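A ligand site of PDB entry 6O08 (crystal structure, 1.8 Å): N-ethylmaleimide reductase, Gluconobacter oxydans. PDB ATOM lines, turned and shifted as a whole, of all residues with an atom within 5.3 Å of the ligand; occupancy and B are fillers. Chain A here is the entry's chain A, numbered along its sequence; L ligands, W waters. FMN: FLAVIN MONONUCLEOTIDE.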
ATOM      1  N   SER A  22      11.131 -17.021 -15.977  1.00  0.00           N
ATOM      2  CA  SER A  22      10.633 -16.929 -14.580  1.00  0.00           C
ATOM      3  C   SER A  22       9.808 -18.185 -14.240  1.00  0.00           C
ATOM      4  O   SER A  22       9.367 -18.936 -15.119  1.00  0.00           O
ATOM      5  CB  SER A  22       9.917 -15.645 -14.323  1.00  0.00           C
ATOM      6  OG  SER A  22       8.532 -15.754 -14.558  1.00  0.00           O
ATOM      7  N   PRO A  23       9.726 -18.518 -12.941  1.00  0.00           N
ATOM      8  CA  PRO A  23       8.999 -19.699 -12.468  1.00  0.00           C
ATOM      9  C   PRO A  23       7.492 -19.547 -12.730  1.00  0.00           C
ATOM     10  O   PRO A  23       6.935 -18.517 -12.344  1.00  0.00           O
ATOM     11  CB  PRO A  23       9.357 -19.733 -10.967  1.00  0.00           C
ATOM     12  CG  PRO A  23       9.662 -18.277 -10.609  1.00  0.00           C
ATOM     13  CD  PRO A  23      10.335 -17.740 -11.837  1.00  0.00           C
ATOM     14  N   LEU A  24       6.878 -20.561 -13.355  1.00  0.00           N
ATOM     15  CA  LEU A  24       5.440 -20.527 -13.752  1.00  0.00           C
ATOM     16  C   LEU A  24       4.774 -21.855 -13.411  1.00  0.00           C
ATOM     17  O   LEU A  24       5.041 -22.801 -14.112  1.00  0.00           O
ATOM     18  CB  LEU A  24       5.321 -20.234 -15.256  1.00  0.00           C
ATOM     19  CG  LEU A  24       5.896 -18.894 -15.686  1.00  0.00           C
ATOM     20  CD1 LEU A  24       6.305 -18.946 -17.154  1.00  0.00           C
ATOM     21  CD2 LEU A  24       4.889 -17.771 -15.425  1.00  0.00           C
ATOM     22  N   THR A  25       3.935 -21.889 -12.381  1.00  0.00           N
ATOM     23  CA  THR A  25       2.971 -22.964 -12.067  1.00  0.00           C
ATOM     24  C   THR A  25       2.048 -23.169 -13.277  1.00  0.00           C
ATOM     25  O   THR A  25       1.463 -22.188 -13.757  1.00  0.00           O
ATOM     26  CB  THR A  25       2.250 -22.646 -10.757  1.00  0.00           C
ATOM     27  OG1 THR A  25       3.205 -22.709  -9.677  1.00  0.00           O
ATOM     28  CG2 THR A  25       1.069 -23.557 -10.506  1.00  0.00           C
ATOM     29  N   ARG A  26       1.949 -24.400 -13.778  1.00  0.00           N
ATOM     30  CA  ARG A  26       1.178 -24.748 -15.004  1.00  0.00           C
ATOM     31  C   ARG A  26       0.200 -25.893 -14.698  1.00  0.00           C
ATOM     32  O   ARG A  26      -0.739 -26.027 -15.457  1.00  0.00           O
ATOM     33  CB  ARG A  26       2.119 -25.052 -16.173  1.00  0.00           C
ATOM     34  CG  ARG A  26       3.176 -23.974 -16.466  1.00  0.00           C
ATOM     35  CD  ARG A  26       2.563 -22.596 -16.709  1.00  0.00           C
ATOM     36  NE  ARG A  26       1.415 -22.601 -17.636  1.00  0.00           N
ATOM     37  CZ  ARG A  26       1.525 -22.546 -18.963  1.00  0.00           C
ATOM     38  NH1 ARG A  26       0.449 -22.604 -19.725  1.00  0.00           N
ATOM     39  NH2 ARG A  26       2.704 -22.452 -19.530  1.00  0.00           N
ATOM     40  N   THR A  54      12.165 -23.478 -12.945  1.00  0.00           N
ATOM     41  CA  THR A  54      10.968 -24.340 -13.033  1.00  0.00           C
ATOM     42  C   THR A  54       9.764 -23.629 -12.399  1.00  0.00           C
ATOM     43  O   THR A  54       9.964 -22.779 -11.493  1.00  0.00           O
ATOM     44  CB  THR A  54      11.158 -25.729 -12.393  1.00  0.00           C
ATOM     45  OG1 THR A  54      11.256 -25.644 -10.972  1.00  0.00           O
ATOM     46  CG2 THR A  54      12.342 -26.465 -12.979  1.00  0.00           C
ATOM     47  N   GLU A  55       8.560 -24.045 -12.804  1.00  0.00           N
ATOM     48  CA  GLU A  55       7.382 -23.972 -11.908  1.00  0.00           C
ATOM     49  C   GLU A  55       7.794 -24.289 -10.460  1.00  0.00           C
ATOM     50  O   GLU A  55       8.694 -25.164 -10.222  1.00  0.00           O
ATOM     51  CB  GLU A  55       6.344 -25.011 -12.317  1.00  0.00           C
ATOM     52  CG  GLU A  55       6.837 -26.435 -12.248  1.00  0.00           C
ATOM     53  CD  GLU A  55       6.157 -27.295 -13.303  1.00  0.00           C
ATOM     54  OE1 GLU A  55       6.788 -27.534 -14.318  1.00  0.00           O
ATOM     55  OE2 GLU A  55       4.964 -27.646 -13.085  1.00  0.00           O
ATOM     56  N   ALA A  56       7.143 -23.657  -9.502  1.00  0.00           N
ATOM     57  CA  ALA A  56       7.289 -23.958  -8.057  1.00  0.00           C
ATOM     58  C   ALA A  56       7.052 -25.455  -7.860  1.00  0.00           C
ATOM     59  O   ALA A  56       6.047 -25.965  -8.390  1.00  0.00           O
ATOM     60  CB  ALA A  56       6.308 -23.136  -7.275  1.00  0.00           C
ATOM     61  N   GLN A  98      12.693 -24.574  -8.590  1.00  0.00           N
ATOM     62  CA  GLN A  98      12.201 -23.627  -7.598  1.00  0.00           C
ATOM     63  C   GLN A  98      11.551 -24.434  -6.479  1.00  0.00           C
ATOM     64  O   GLN A  98      10.542 -25.132  -6.746  1.00  0.00           O
ATOM     65  CB  GLN A  98      11.207 -22.623  -8.207  1.00  0.00           C
ATOM     66  CG  GLN A  98      10.840 -21.593  -7.167  1.00  0.00           C
ATOM     67  CD  GLN A  98       9.737 -20.638  -7.513  1.00  0.00           C
ATOM     68  OE1 GLN A  98       8.600 -21.045  -7.778  1.00  0.00           O
ATOM     69  NE2 GLN A  98      10.044 -19.353  -7.370  1.00  0.00           N
ATOM     70  N   TRP A 100       9.377 -25.100  -3.272  1.00  0.00           N
ATOM     71  CA  TRP A 100       8.122 -24.512  -2.780  1.00  0.00           C
ATOM     72  C   TRP A 100       7.649 -25.143  -1.479  1.00  0.00           C
ATOM     73  O   TRP A 100       7.383 -26.362  -1.443  1.00  0.00           O
ATOM     74  CB  TRP A 100       7.065 -24.764  -3.838  1.00  0.00           C
ATOM     75  CG  TRP A 100       5.971 -23.775  -3.905  1.00  0.00           C
ATOM     76  CD1 TRP A 100       5.867 -22.544  -3.346  1.00  0.00           C
ATOM     77  CD2 TRP A 100       4.827 -23.954  -4.744  1.00  0.00           C
ATOM     78  NE1 TRP A 100       4.703 -21.941  -3.770  1.00  0.00           N
ATOM     79  CE2 TRP A 100       4.070 -22.768  -4.665  1.00  0.00           C
ATOM     80  CE3 TRP A 100       4.397 -24.981  -5.585  1.00  0.00           C
ATOM     81  CZ2 TRP A 100       2.896 -22.598  -5.395  1.00  0.00           C
ATOM     82  CZ3 TRP A 100       3.253 -24.809  -6.328  1.00  0.00           C
ATOM     83  CH2 TRP A 100       2.498 -23.642  -6.213  1.00  0.00           C
ATOM     84  N   HIS A 172      11.913 -20.564  -3.024  1.00  0.00           N
ATOM     85  CA  HIS A 172      10.731 -19.689  -3.215  1.00  0.00           C
ATOM     86  C   HIS A 172      10.465 -19.042  -1.864  1.00  0.00           C
ATOM     87  O   HIS A 172       9.971 -19.747  -0.979  1.00  0.00           O
ATOM     88  CB  HIS A 172       9.553 -20.463  -3.784  1.00  0.00           C
ATOM     89  CG  HIS A 172       8.455 -19.570  -4.253  1.00  0.00           C
ATOM     90  ND1 HIS A 172       8.332 -18.264  -3.796  1.00  0.00           N
ATOM     91  CD2 HIS A 172       7.419 -19.779  -5.093  1.00  0.00           C
ATOM     92  CE1 HIS A 172       7.265 -17.722  -4.365  1.00  0.00           C
ATOM     93  NE2 HIS A 172       6.687 -18.647  -5.158  1.00  0.00           N
ATOM     94  N   ASN A 175       5.801 -14.203  -2.647  1.00  0.00           N
ATOM     95  CA  ASN A 175       4.384 -14.380  -3.063  1.00  0.00           C
ATOM     96  C   ASN A 175       3.546 -14.965  -1.921  1.00  0.00           C
ATOM     97  O   ASN A 175       2.557 -15.691  -2.199  1.00  0.00           O
ATOM     98  CB  ASN A 175       4.312 -15.205  -4.355  1.00  0.00           C
ATOM     99  CG  ASN A 175       5.135 -14.605  -5.490  1.00  0.00           C
ATOM    100  OD1 ASN A 175       5.499 -13.428  -5.457  1.00  0.00           O
ATOM    101  ND2 ASN A 175       5.456 -15.418  -6.486  1.00  0.00           N
ATOM    102  N   ARG A 224      14.307 -16.275  -4.476  1.00  0.00           N
ATOM    103  CA  ARG A 224      13.336 -15.286  -4.956  1.00  0.00           C
ATOM    104  C   ARG A 224      12.693 -14.599  -3.764  1.00  0.00           C
ATOM    105  O   ARG A 224      12.160 -15.273  -2.855  1.00  0.00           O
ATOM    106  CB  ARG A 224      12.275 -15.945  -5.854  1.00  0.00           C
ATOM    107  CG  ARG A 224      11.225 -14.954  -6.354  1.00  0.00           C
ATOM    108  CD  ARG A 224      10.134 -15.599  -7.212  1.00  0.00           C
ATOM    109  NE  ARG A 224      10.304 -15.255  -8.614  1.00  0.00           N
ATOM    110  CZ  ARG A 224       9.313 -14.912  -9.456  1.00  0.00           C
ATOM    111  NH1 ARG A 224       8.054 -14.886  -9.044  1.00  0.00           N
ATOM    112  NH2 ARG A 224       9.614 -14.580 -10.690  1.00  0.00           N
ATOM    113  N   ARG A 261      10.924 -10.054  -7.609  1.00  0.00           N
ATOM    114  CA  ARG A 261       9.653  -9.777  -8.307  1.00  0.00           C
ATOM    115  C   ARG A 261       9.154  -8.452  -7.722  1.00  0.00           C
ATOM    116  O   ARG A 261       8.930  -8.397  -6.539  1.00  0.00           O
ATOM    117  CB  ARG A 261       8.624 -10.882  -8.087  1.00  0.00           C
ATOM    118  CG  ARG A 261       7.321 -10.670  -8.830  1.00  0.00           C
ATOM    119  CD  ARG A 261       6.241 -11.596  -8.345  1.00  0.00           C
ATOM    120  NE  ARG A 261       4.940 -10.999  -8.503  1.00  0.00           N
ATOM    121  CZ  ARG A 261       4.147 -10.630  -7.493  1.00  0.00           C
ATOM    122  NH1 ARG A 261       2.983 -10.077  -7.743  1.00  0.00           N
ATOM    123  NH2 ARG A 261       4.502 -10.828  -6.235  1.00  0.00           N
ATOM    124  N   PHE A 269       0.435  -8.086 -12.883  1.00  0.00           N
ATOM    125  CA  PHE A 269       0.424  -9.276 -11.995  1.00  0.00           C
ATOM    126  C   PHE A 269       0.693  -8.788 -10.570  1.00  0.00           C
ATOM    127  O   PHE A 269       1.494  -9.361  -9.839  1.00  0.00           O
ATOM    128  CB  PHE A 269       1.458 -10.292 -12.492  1.00  0.00           C
ATOM    129  CG  PHE A 269       1.231 -11.692 -12.008  1.00  0.00           C
ATOM    130  CD1 PHE A 269       0.337 -12.525 -12.662  1.00  0.00           C
ATOM    131  CD2 PHE A 269       1.903 -12.188 -10.905  1.00  0.00           C
ATOM    132  CE1 PHE A 269       0.121 -13.814 -12.202  1.00  0.00           C
ATOM    133  CE2 PHE A 269       1.700 -13.487 -10.471  1.00  0.00           C
ATOM    134  CZ  PHE A 269       0.808 -14.289 -11.116  1.00  0.00           C
ATOM    135  N   ASN A 292      12.295  -8.900 -12.197  1.00  0.00           N
ATOM    136  CA  ASN A 292      11.132  -9.523 -12.831  1.00  0.00           C
ATOM    137  C   ASN A 292       9.912  -8.661 -12.550  1.00  0.00           C
ATOM    138  O   ASN A 292       9.863  -8.029 -11.462  1.00  0.00           O
ATOM    139  CB  ASN A 292      10.905 -10.938 -12.279  1.00  0.00           C
ATOM    140  CG  ASN A 292       9.534 -11.465 -12.587  1.00  0.00           C
ATOM    141  OD1 ASN A 292       8.643 -11.337 -11.746  1.00  0.00           O
ATOM    142  ND2 ASN A 292       9.325 -11.930 -13.826  1.00  0.00           N
ATOM    143  N   GLN A 293       9.011  -8.663 -13.530  1.00  0.00           N
ATOM    144  CA  GLN A 293       7.579  -8.252 -13.511  1.00  0.00           C
ATOM    145  C   GLN A 293       7.416  -7.073 -14.484  1.00  0.00           C
ATOM    146  O   GLN A 293       8.105  -6.040 -14.324  1.00  0.00           O
ATOM    147  CB  GLN A 293       7.061  -7.933 -12.113  1.00  0.00           C
ATOM    148  CG  GLN A 293       5.647  -7.362 -12.158  1.00  0.00           C
ATOM    149  CD  GLN A 293       4.636  -8.113 -11.342  1.00  0.00           C
ATOM    150  OE1 GLN A 293       4.950  -9.065 -10.619  1.00  0.00           O
ATOM    151  NE2 GLN A 293       3.393  -7.658 -11.462  1.00  0.00           N
ATOM    152  N   ASP A 294       6.563  -7.261 -15.500  1.00  0.00           N
ATOM    153  CA  ASP A 294       6.208  -6.275 -16.553  1.00  0.00           C
ATOM    154  C   ASP A 294       7.430  -5.807 -17.348  1.00  0.00           C
ATOM    155  O   ASP A 294       7.338  -4.745 -17.924  1.00  0.00           O
ATOM    156  CB  ASP A 294       5.470  -5.089 -15.912  1.00  0.00           C
ATOM    157  CG  ASP A 294       4.190  -5.484 -15.194  1.00  0.00           C
ATOM    158  OD1 ASP A 294       3.521  -6.363 -15.691  1.00  0.00           O
ATOM    159  OD2 ASP A 294       3.886  -4.907 -14.150  1.00  0.00           O
ATOM    160  N   TYR A 295       8.548  -6.531 -17.432  1.00  0.00           N
ATOM    161  CA  TYR A 295       9.674  -6.108 -18.300  1.00  0.00           C
ATOM    162  C   TYR A 295       9.293  -6.323 -19.771  1.00  0.00           C
ATOM    163  O   TYR A 295       8.637  -7.262 -20.119  1.00  0.00           O
ATOM    164  CB  TYR A 295      10.992  -6.789 -17.938  1.00  0.00           C
ATOM    165  CG  TYR A 295      11.651  -6.102 -16.760  1.00  0.00           C
ATOM    166  CD1 TYR A 295      12.519  -5.037 -16.960  1.00  0.00           C
ATOM    167  CD2 TYR A 295      11.328  -6.452 -15.455  1.00  0.00           C
ATOM    168  CE1 TYR A 295      13.069  -4.350 -15.883  1.00  0.00           C
ATOM    169  CE2 TYR A 295      11.841  -5.753 -14.370  1.00  0.00           C
ATOM    170  CZ  TYR A 295      12.741  -4.707 -14.589  1.00  0.00           C
ATOM    171  OH  TYR A 295      13.310  -4.029 -13.559  1.00  0.00           O
ATOM    172  N   ALA A 313      14.084 -11.760 -15.731  1.00  0.00           N
ATOM    173  CA  ALA A 313      13.238 -12.957 -15.864  1.00  0.00           C
ATOM    174  C   ALA A 313      11.894 -12.507 -16.421  1.00  0.00           C
ATOM    175  O   ALA A 313      11.329 -11.509 -15.928  1.00  0.00           O
ATOM    176  CB  ALA A 313      13.123 -13.688 -14.544  1.00  0.00           C
ATOM    177  N   PHE A 314      11.416 -13.246 -17.438  1.00  0.00           N
ATOM    178  CA  PHE A 314      10.118 -13.028 -18.117  1.00  0.00           C
ATOM    179  C   PHE A 314       9.227 -14.228 -17.816  1.00  0.00           C
ATOM    180  O   PHE A 314       9.657 -15.400 -18.026  1.00  0.00           O
ATOM    181  CB  PHE A 314      10.366 -12.869 -19.611  1.00  0.00           C
ATOM    182  CG  PHE A 314      11.320 -11.757 -19.976  1.00  0.00           C
ATOM    183  CD1 PHE A 314      12.693 -11.957 -20.002  1.00  0.00           C
ATOM    184  CD2 PHE A 314      10.835 -10.485 -20.265  1.00  0.00           C
ATOM    185  CE1 PHE A 314      13.545 -10.926 -20.365  1.00  0.00           C
ATOM    186  CE2 PHE A 314      11.683  -9.447 -20.605  1.00  0.00           C
ATOM    187  CZ  PHE A 314      13.044  -9.672 -20.646  1.00  0.00           C
ATOM    188  N   GLY A 315       8.030 -13.965 -17.294  1.00  0.00           N
ATOM    189  CA  GLY A 315       7.040 -15.018 -17.034  1.00  0.00           C
ATOM    190  C   GLY A 315       6.101 -15.191 -18.212  1.00  0.00           C
ATOM    191  O   GLY A 315       6.301 -16.110 -19.012  1.00  0.00           O
ATOM    192  N   ARG A 316       5.081 -14.360 -18.290  1.00  0.00           N
ATOM    193  CA  ARG A 316       3.968 -14.556 -19.253  1.00  0.00           C
ATOM    194  C   ARG A 316       4.484 -14.605 -20.682  1.00  0.00           C
ATOM    195  O   ARG A 316       3.955 -15.385 -21.473  1.00  0.00           O
ATOM    196  CB  ARG A 316       2.931 -13.454 -19.045  1.00  0.00           C
ATOM    197  CG  ARG A 316       2.124 -13.686 -17.770  1.00  0.00           C
ATOM    198  CD  ARG A 316       1.385 -12.466 -17.277  1.00  0.00           C
ATOM    199  NE  ARG A 316       2.298 -11.425 -16.757  1.00  0.00           N
ATOM    200  CZ  ARG A 316       1.905 -10.213 -16.395  1.00  0.00           C
ATOM    201  NH1 ARG A 316       0.602  -9.911 -16.455  1.00  0.00           N
ATOM    202  NH2 ARG A 316       2.836  -9.295 -15.943  1.00  0.00           N
ATOM    203  N   LYS A 317       5.492 -13.824 -21.029  1.00  0.00           N
ATOM    204  CA  LYS A 317       6.016 -13.821 -22.404  1.00  0.00           C
ATOM    205  C   LYS A 317       6.561 -15.227 -22.755  1.00  0.00           C
ATOM    206  O   LYS A 317       6.408 -15.644 -23.914  1.00  0.00           O
ATOM    207  CB  LYS A 317       7.053 -12.717 -22.583  1.00  0.00           C
ATOM    208  CG  LYS A 317       6.480 -11.305 -22.655  1.00  0.00           C
ATOM    209  CD  LYS A 317       7.570 -10.264 -22.691  1.00  0.00           C
ATOM    210  CE  LYS A 317       7.123  -8.909 -23.223  1.00  0.00           C
ATOM    211  NZ  LYS A 317       5.956  -8.425 -22.468  1.00  0.00           N
ATOM    212  N   ILE A 319       5.372 -18.036 -21.590  1.00  0.00           N
ATOM    213  CA  ILE A 319       4.213 -18.949 -21.812  1.00  0.00           C
ATOM    214  C   ILE A 319       3.970 -19.109 -23.329  1.00  0.00           C
ATOM    215  O   ILE A 319       3.775 -20.268 -23.839  1.00  0.00           O
ATOM    216  CB  ILE A 319       2.975 -18.414 -21.065  1.00  0.00           C
ATOM    217  CG1 ILE A 319       3.196 -18.441 -19.555  1.00  0.00           C
ATOM    218  CG2 ILE A 319       1.731 -19.146 -21.509  1.00  0.00           C
ATOM    219  CD1 ILE A 319       2.047 -17.877 -18.748  1.00  0.00           C
ATOM    220  N   TRP A 342      -3.574 -21.080 -18.404  1.00  0.00           N
ATOM    221  CA  TRP A 342      -2.424 -20.978 -17.472  1.00  0.00           C
ATOM    222  C   TRP A 342      -2.301 -22.255 -16.625  1.00  0.00           C
ATOM    223  O   TRP A 342      -1.159 -22.779 -16.469  1.00  0.00           O
ATOM    224  CB  TRP A 342      -2.515 -19.756 -16.552  1.00  0.00           C
ATOM    225  CG  TRP A 342      -2.165 -18.454 -17.203  1.00  0.00           C
ATOM    226  CD1 TRP A 342      -1.643 -18.262 -18.442  1.00  0.00           C
ATOM    227  CD2 TRP A 342      -2.179 -17.165 -16.567  1.00  0.00           C
ATOM    228  NE1 TRP A 342      -1.389 -16.934 -18.645  1.00  0.00           N
ATOM    229  CE2 TRP A 342      -1.686 -16.239 -17.507  1.00  0.00           C
ATOM    230  CE3 TRP A 342      -2.580 -16.696 -15.310  1.00  0.00           C
ATOM    231  CZ2 TRP A 342      -1.582 -14.870 -17.241  1.00  0.00           C
ATOM    232  CZ3 TRP A 342      -2.483 -15.346 -15.048  1.00  0.00           C
ATOM    233  CH2 TRP A 342      -2.003 -14.444 -16.003  1.00  0.00           C
ATOM    234  N   TYR A 343      -3.430 -22.723 -16.093  1.00  0.00           N
ATOM    235  CA  TYR A 343      -3.477 -23.735 -15.005  1.00  0.00           C
ATOM    236  C   TYR A 343      -4.368 -24.921 -15.358  1.00  0.00           C
ATOM    237  O   TYR A 343      -4.640 -25.720 -14.443  1.00  0.00           O
ATOM    238  CB  TYR A 343      -3.983 -23.140 -13.689  1.00  0.00           C
ATOM    239  CG  TYR A 343      -3.262 -21.906 -13.206  1.00  0.00           C
ATOM    240  CD1 TYR A 343      -1.895 -21.908 -12.979  1.00  0.00           C
ATOM    241  CD2 TYR A 343      -3.971 -20.753 -12.913  1.00  0.00           C
ATOM    242  CE1 TYR A 343      -1.234 -20.778 -12.516  1.00  0.00           C
ATOM    243  CE2 TYR A 343      -3.337 -19.616 -12.435  1.00  0.00           C
ATOM    244  CZ  TYR A 343      -1.970 -19.634 -12.232  1.00  0.00           C
ATOM    245  OH  TYR A 343      -1.371 -18.505 -11.752  1.00  0.00           O
HETATM  246  N1  FMN L   1       6.062 -17.090  -9.394  1.00  0.00           N
HETATM  247  C2  FMN L   1       6.773 -18.007  -8.683  1.00  0.00           C
HETATM  248  O2  FMN L   1       7.674 -17.607  -7.919  1.00  0.00           O
HETATM  249  N3  FMN L   1       6.527 -19.336  -8.732  1.00  0.00           N
HETATM  250  C4  FMN L   1       5.577 -19.867  -9.515  1.00  0.00           C
HETATM  251  O4  FMN L   1       5.377 -21.076  -9.589  1.00  0.00           O
HETATM  252  C4A FMN L   1       4.777 -18.961 -10.364  1.00  0.00           C
HETATM  253  N5  FMN L   1       3.806 -19.411 -11.174  1.00  0.00           N
HETATM  254  C5A FMN L   1       3.175 -18.535 -11.991  1.00  0.00           C
HETATM  255  C6  FMN L   1       2.249 -19.016 -12.889  1.00  0.00           C
HETATM  256  C7  FMN L   1       1.532 -18.155 -13.730  1.00  0.00           C
HETATM  257  C7M FMN L   1       0.510 -18.748 -14.698  1.00  0.00           C
HETATM  258  C8  FMN L   1       1.823 -16.721 -13.742  1.00  0.00           C
HETATM  259  C8M FMN L   1       1.075 -15.726 -14.637  1.00  0.00           C
HETATM  260  C9  FMN L   1       2.769 -16.215 -12.840  1.00  0.00           C
HETATM  261  C9A FMN L   1       3.466 -17.084 -11.978  1.00  0.00           C
HETATM  262  N10 FMN L   1       4.461 -16.601 -11.109  1.00  0.00           N
HETATM  263  C10 FMN L   1       5.125 -17.516 -10.276  1.00  0.00           C
HETATM  264  C1' FMN L   1       4.855 -15.204 -11.082  1.00  0.00           C
HETATM  265  C2' FMN L   1       5.839 -15.115 -12.274  1.00  0.00           C
HETATM  266  O2' FMN L   1       7.093 -15.811 -12.127  1.00  0.00           O
HETATM  267  C3' FMN L   1       6.248 -13.669 -12.591  1.00  0.00           C
HETATM  268  O3' FMN L   1       6.834 -13.144 -11.396  1.00  0.00           O
HETATM  269  C4' FMN L   1       5.046 -12.836 -13.052  1.00  0.00           C
HETATM  270  O4' FMN L   1       4.362 -13.520 -14.152  1.00  0.00           O
HETATM  271  C5' FMN L   1       5.533 -11.441 -13.424  1.00  0.00           C
HETATM  272  O5' FMN L   1       6.464 -11.507 -14.515  1.00  0.00           O
HETATM  273  P   FMN L   1       6.006 -11.172 -16.057  1.00  0.00           P
HETATM  274  O1P FMN L   1       7.324 -11.277 -16.812  1.00  0.00           O
HETATM  275  O2P FMN L   1       5.478  -9.740 -16.004  1.00  0.00           O
HETATM  276  O3P FMN L   1       4.921 -12.212 -16.334  1.00  0.00           O
HETATM  277  O   HOH W   1       9.195  -9.565 -16.402  1.00  0.00           O
HETATM  278  O   HOH W   2       6.810 -11.586 -19.452  1.00  0.00           O
HETATM  279  O   HOH W   3       4.742  -9.085 -18.549  1.00  0.00           O
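OE1 of Gln 98 lies close to N of Ala 56, at 3.5 Å. The backbone carbonyl oxygen (O) of Phe 269 is in hydrogen-bond range of the side-chain amide nitrogen (NE2) of Gln 293 (3.0 Å). O of Trp 342 sits at hydrogen-bond distance from NE of Arg 26 (2.8 Å). The backbone NH (N) of Gln 98 lies within hydrogen-bond range of the side-chain hydroxyl (OG1) of Thr 54 (3.0 Å). The guanidinium group (NH2) of Arg 316 lies within salt-bridge range of the side-chain carboxylate (OD1) of Asp 294, 3.0 Å away. The backbone carbonyl oxygen of Phe 269 is in hydrogen-bond range of the guanidinium group of Arg 261, at 2.7 Å. The guanidinium group (NE) of Arg 261 lies within hydrogen-bond range of the side-chain amide oxygen (OE1) of Gln 293, 2.9 Å away. ND2 of Asn 292 lies within hydrogen-bond range of O of Ala 313 (2.9 Å).
Water W3 bridges O2P of the ligand (2.7 Å) and NH2 of Arg 316 (3.2 Å).
Residues that only touch the ligand: Leu 24 (3.2 Å), Arg 261 (3.5 Å), Phe 269 (3.2 Å), Gln 293 (3.6 Å), Phe 314 (3.5 Å), Trp 342 (3.6 Å) and Tyr 343 (3.5 Å). Hydrophobic or aromatic side chains within 4 Å of the ligand: Pro 23, Leu 24, Ala 56, His 172, Phe 269, Trp 342 and Tyr 343. Of the 27 residues printed, 19 come within 4 Å of the ligand.
The side-chain hydroxyl (OG) of Ser 22 sits at hydrogen-bond distance from an oxygen (O2') of the ligand, at 2.8 Å. The side-chain amide nitrogen (ND2) of Asn 175 sits at hydrogen-bond distance from a nitrogen (N1) of the ligand, 3.4 Å away. N5 of the ligand is in hydrogen-bond range of N of Thr 25, at 2.8 Å. An oxygen (O2) of the ligand sits at hydrogen-bond distance from the guanidinium group (NH1) of Arg 224, 3.0 Å away. An oxygen (O4) of the ligand sits at hydrogen-bond distance from the backbone NH of Ala 56, at 3.1 Å. An oxygen (O3') of the ligand sits at hydrogen-bond distance from the side-chain amide oxygen of Asn 292, 2.6 Å away. An oxygen (O1P) of the ligand sits at hydrogen-bond distance from the backbone NH (N) of Gly 315, 2.8 Å away. O of Pro 23 lies within hydrogen-bond range of O2' of the ligand (2.7 Å). N of Arg 316 sits at hydrogen-bond distance from O3P of the ligand (2.9 Å). The side-chain amide oxygen (OE1) of Gln 98 lies within hydrogen-bond range of a nitrogen (N3) of the ligand (2.9 Å). The guanidinium group of Arg 316 is in salt-bridge range of an oxygen (O2P) of the ligand, at 2.7 Å. An oxygen (O4) of the ligand lies within hydrogen-bond range of the side-chain hydroxyl of Thr 25 (2.7 Å). N of Asp 294 sits at hydrogen-bond distance from O2P of the ligand (2.8 Å). A ring nitrogen (NE2) of His 172 is in hydrogen-bond range of an oxygen (O2) of the ligand, at 3.1 Å.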
